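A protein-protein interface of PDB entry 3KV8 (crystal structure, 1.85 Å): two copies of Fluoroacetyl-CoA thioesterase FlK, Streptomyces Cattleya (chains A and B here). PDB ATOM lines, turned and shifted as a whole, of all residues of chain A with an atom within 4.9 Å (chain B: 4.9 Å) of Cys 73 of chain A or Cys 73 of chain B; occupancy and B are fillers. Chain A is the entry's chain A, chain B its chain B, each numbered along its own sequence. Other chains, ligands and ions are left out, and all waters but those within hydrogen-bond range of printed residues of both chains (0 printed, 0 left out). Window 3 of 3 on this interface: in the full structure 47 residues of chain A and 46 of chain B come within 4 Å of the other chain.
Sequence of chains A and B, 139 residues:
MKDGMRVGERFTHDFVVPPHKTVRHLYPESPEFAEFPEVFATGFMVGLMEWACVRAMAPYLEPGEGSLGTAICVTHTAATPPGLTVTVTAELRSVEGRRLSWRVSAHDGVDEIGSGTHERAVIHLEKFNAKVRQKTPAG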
ATOM      1  N   ALA A  71      -2.468  -1.430  16.420  1.00  0.00           N
ATOM      2  CA  ALA A  71      -3.819  -0.880  16.712  1.00  0.00           C
ATOM      3  C   ALA A  71      -4.423  -0.245  15.471  1.00  0.00           C
ATOM      4  O   ALA A  71      -3.730   0.429  14.690  1.00  0.00           O
ATOM      5  CB  ALA A  71      -3.787   0.132  17.840  1.00  0.00           C
ATOM      6  N   ILE A  72      -5.734  -0.380  15.343  1.00  0.00           N
ATOM      7  CA  ILE A  72      -6.432   0.341  14.247  1.00  0.00           C
ATOM      8  C   ILE A  72      -7.722   0.925  14.864  1.00  0.00           C
ATOM      9  O   ILE A  72      -8.462   0.211  15.548  1.00  0.00           O
ATOM     10  CB  ILE A  72      -6.678  -0.588  13.007  1.00  0.00           C
ATOM     11  CG1 ILE A  72      -7.326   0.230  11.858  1.00  0.00           C
ATOM     12  CG2 ILE A  72      -7.616  -1.829  13.393  1.00  0.00           C
ATOM     13  CD1 ILE A  72      -6.368   1.204  11.148  1.00  0.00           C
ATOM     14  N   CYS A  73      -7.938   2.237  14.726  1.00  0.00           N
ATOM     15  CA  CYS A  73      -9.110   2.858  15.302  1.00  0.00           C
ATOM     16  C   CYS A  73      -9.719   3.785  14.242  1.00  0.00           C
ATOM     17  O   CYS A  73      -9.292   4.925  14.067  1.00  0.00           O
ATOM     18  CB  CYS A  73      -8.805   3.560  16.678  1.00  0.00           C
ATOM     19  SG  CYS A  73     -10.277   4.166  17.483  1.00  0.00           S
ATOM     20  N   VAL A  74     -10.727   3.276  13.519  1.00  0.00           N
ATOM     21  CA  VAL A  74     -11.260   4.010  12.365  1.00  0.00           C
ATOM     22  C   VAL A  74     -12.777   3.912  12.242  1.00  0.00           C
ATOM     23  O   VAL A  74     -13.406   2.889  12.663  1.00  0.00           O
ATOM     24  CB  VAL A  74     -10.663   3.593  10.967  1.00  0.00           C
ATOM     25  CG1 VAL A  74      -9.196   3.835  10.938  1.00  0.00           C
ATOM     26  CG2 VAL A  74     -10.932   2.103  10.685  1.00  0.00           C
ATOM     27  N   THR A  75     -13.340   4.907  11.544  1.00  0.00           N
ATOM     28  CA  THR A  75     -14.750   4.826  11.193  1.00  0.00           C
ATOM     29  C   THR A  75     -14.802   4.320   9.716  1.00  0.00           C
ATOM     30  O   THR A  75     -13.801   4.412   8.982  1.00  0.00           O
ATOM     31  CB  THR A  75     -15.413   6.228  11.208  1.00  0.00           C
ATOM     32  OG1 THR A  75     -14.617   7.119  10.452  1.00  0.00           O
ATOM     33  CG2 THR A  75     -15.503   6.813  12.632  1.00  0.00           C
ATOM     34  N   SER A 115     -11.931   7.339   8.630  1.00  0.00           N
ATOM     35  CA  SER A 115     -10.708   7.986   9.092  1.00  0.00           C
ATOM     36  C   SER A 115     -10.452   7.548  10.575  1.00  0.00           C
ATOM     37  O   SER A 115     -11.357   7.034  11.232  1.00  0.00           O
ATOM     38  CB  SER A 115     -10.868   9.513   8.978  1.00  0.00           C
ATOM     39  OG  SER A 115     -11.622  10.076  10.092  1.00  0.00           O
ATOM     40  N   GLY A 116      -9.227   7.725  11.061  1.00  0.00           N
ATOM     41  CA  GLY A 116      -8.926   7.468  12.501  1.00  0.00           C
ATOM     42  C   GLY A 116      -7.414   7.332  12.579  1.00  0.00           C
ATOM     43  O   GLY A 116      -6.734   8.107  11.995  1.00  0.00           O
ATOM     44  N   THR A 117      -6.924   6.386  13.361  1.00  0.00           N
ATOM     45  CA  THR A 117      -5.529   6.256  13.662  1.00  0.00           C
ATOM     46  C   THR A 117      -5.088   4.819  13.490  1.00  0.00           C
ATOM     47  O   THR A 117      -5.869   3.848  13.560  1.00  0.00           O
ATOM     48  CB  THR A 117      -5.262   6.747  15.155  1.00  0.00           C
ATOM     49  OG1 THR A 117      -6.159   6.074  16.055  1.00  0.00           O
ATOM     50  CG2 THR A 117      -5.441   8.194  15.241  1.00  0.00           C
ATOM     51  N   ALA B  71     -17.533   1.260  12.410  1.00  0.00           N
ATOM     52  CA  ALA B  71     -16.349   1.687  13.150  1.00  0.00           C
ATOM     53  C   ALA B  71     -15.724   0.443  13.767  1.00  0.00           C
ATOM     54  O   ALA B  71     -16.428  -0.531  14.123  1.00  0.00           O
ATOM     55  CB  ALA B  71     -16.764   2.679  14.259  1.00  0.00           C
ATOM     56  N   ILE B  72     -14.404   0.448  13.866  1.00  0.00           N
ATOM     57  CA  ILE B  72     -13.671  -0.658  14.535  1.00  0.00           C
ATOM     58  C   ILE B  72     -12.576   0.087  15.331  1.00  0.00           C
ATOM     59  O   ILE B  72     -12.006   1.074  14.840  1.00  0.00           O
ATOM     60  CB  ILE B  72     -13.123  -1.716  13.546  1.00  0.00           C
ATOM     61  CG1 ILE B  72     -12.443  -2.898  14.267  1.00  0.00           C
ATOM     62  CG2 ILE B  72     -12.141  -1.126  12.478  1.00  0.00           C
ATOM     63  CD1 ILE B  72     -13.427  -3.693  15.026  1.00  0.00           C
ATOM     64  N   CYS B  73     -12.349  -0.282  16.594  1.00  0.00           N
ATOM     65  CA  CYS B  73     -11.272   0.374  17.327  1.00  0.00           C
ATOM     66  C   CYS B  73     -10.668  -0.709  18.233  1.00  0.00           C
ATOM     67  O   CYS B  73     -11.159  -0.940  19.355  1.00  0.00           O
ATOM     68  CB  CYS B  73     -11.820   1.519  18.221  1.00  0.00           C
ATOM     69  SG  CYS B  73     -10.628   2.736  18.957  1.00  0.00           S
ATOM     70  N   VAL B  74      -9.583  -1.297  17.757  1.00  0.00           N
ATOM     71  CA  VAL B  74      -9.030  -2.501  18.444  1.00  0.00           C
ATOM     72  C   VAL B  74      -7.508  -2.438  18.479  1.00  0.00           C
ATOM     73  O   VAL B  74      -6.850  -1.830  17.577  1.00  0.00           O
ATOM     74  CB  VAL B  74      -9.506  -3.862  17.770  1.00  0.00           C
ATOM     75  CG1 VAL B  74     -11.035  -4.102  17.968  1.00  0.00           C
ATOM     76  CG2 VAL B  74      -9.063  -3.975  16.203  1.00  0.00           C
ATOM     77  N   THR B  75      -6.931  -3.033  19.518  1.00  0.00           N
ATOM     78  CA  THR B  75      -5.522  -3.368  19.495  1.00  0.00           C
ATOM     79  C   THR B  75      -5.274  -4.687  18.779  1.00  0.00           C
ATOM     80  O   THR B  75      -6.232  -5.497  18.533  1.00  0.00           O
ATOM     81  CB  THR B  75      -5.034  -3.524  20.976  1.00  0.00           C
ATOM     82  OG1 THR B  75      -5.800  -4.586  21.581  1.00  0.00           O
ATOM     83  CG2 THR B  75      -5.334  -2.197  21.730  1.00  0.00           C
ATOM     84  N   SER B 115      -8.304  -6.423  21.365  1.00  0.00           N
ATOM     85  CA  SER B 115      -9.626  -6.044  21.889  1.00  0.00           C
ATOM     86  C   SER B 115      -9.986  -4.614  21.665  1.00  0.00           C
ATOM     87  O   SER B 115      -9.138  -3.744  21.440  1.00  0.00           O
ATOM     88  CB  SER B 115      -9.783  -6.404  23.398  1.00  0.00           C
ATOM     89  OG  SER B 115      -8.734  -5.769  24.000  1.00  0.00           O
ATOM     90  N   GLY B 116     -11.290  -4.342  21.759  1.00  0.00           N
ATOM     91  CA  GLY B 116     -11.734  -2.958  21.736  1.00  0.00           C
ATOM     92  C   GLY B 116     -13.206  -2.972  21.386  1.00  0.00           C
ATOM     93  O   GLY B 116     -13.991  -3.773  21.936  1.00  0.00           O
ATOM     94  N   THR B 117     -13.574  -2.080  20.472  1.00  0.00           N
ATOM     95  CA  THR B 117     -14.978  -1.827  20.218  1.00  0.00           C
ATOM     96  C   THR B 117     -15.301  -1.929  18.720  1.00  0.00           C
ATOM     97  O   THR B 117     -14.430  -1.794  17.827  1.00  0.00           O
ATOM     98  CB  THR B 117     -15.409  -0.455  20.773  1.00  0.00           C
ATOM     99  OG1 THR B 117     -14.554   0.590  20.268  1.00  0.00           O
ATOM    100  CG2 THR B 117     -15.387  -0.398  22.326  1.00  0.00           C
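The backbone carbonyl oxygen (O) of Val 74 of chain B lies within hydrogen-bond range of the backbone NH (N) of Ile 72 of chain A. The side-chain sulfur (SG) of Cys 73 of chain A forms a disulfide with the side-chain sulfur (SG) of Cys 73 of chain B. O of Ile 72 of chain B lies within hydrogen-bond range of N of Val 74 of chain A (2.9 Å).
N of Cys 73 of chain A lies within hydrogen-bond range of O of Thr 117 of chain A, 2.9 Å away. N of Cys 73 of chain B is in hydrogen-bond range of O of Thr 117 of chain B, 2.9 Å away.
Among the printed residues, merely in contact across the chains: Val 74 of chain A with Ala 71 of chain B (3.2 Å), Ala 71 of chain A with Val 74 of chain B (3.3 Å), Ile 72 of chain A with Cys 73 of chain B (3.3 Å), Cys 73 of chain A with Ile 72 of chain B (3.4 Å) and Ile 72 of chain A with Ile 72 of chain B (3.7 Å).
Printed residues of chain B within 4 Å of Ala 71 of chain A: Val 74. Of the printed residues of chain B, Ile 72 of chain A touches Ile 72, Cys 73 and Val 74. Cys 73 of chain A touches just these residues of chain B: Ile 72 (3.4 Å) and Cys 73 (2.1 Å). Printed residues of chain B within 4 Å of Val 74 of chain A: Ala 71 and Ile 72. Thr 117 of chain A touches none of the printed residues of chain B. Of the printed residues of chain A, Ala 71 of chain B touches Val 74 (3.2 Å). Cys 73 of chain B touches just these residues of chain A: Ile 72 (3.3 Å) and Cys 73 (2.1 Å). Of the printed residues of chain A, Val 74 of chain B touches Ala 71 (3.3 Å) and Ile 72 (2.9 Å). Thr 117 of chain B touches none of the printed residues of chain A.
Hydrophobic or aromatic side chains of chain B that line the printed part of chain A: Ala 71, Ile 72 and Val 74. Hydrophobic or aromatic side chains of chain A within 4 Å of the printed part of chain B: Ala 71, Ile 72 and Val 74. Among the printed residues, no Asp or Glu carboxylate lies within 4 Å of a Lys or Arg side-chain nitrogen of the other chain.
Ala 71 of chain A touches Val 74 of chain B, and with the chains exchanged Val 74 of chain A touches Ala 71 of chain B. Ile 72 of chain A touches its own counterpart, Ile 72 of chain B. Ile 72 of chain A touches Cys 73 of chain B, and with the chains exchanged Cys 73 of chain A touches Ile 72 of chain B. Cys 73 of chain A touches its own counterpart, Cys 73 of chain B.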
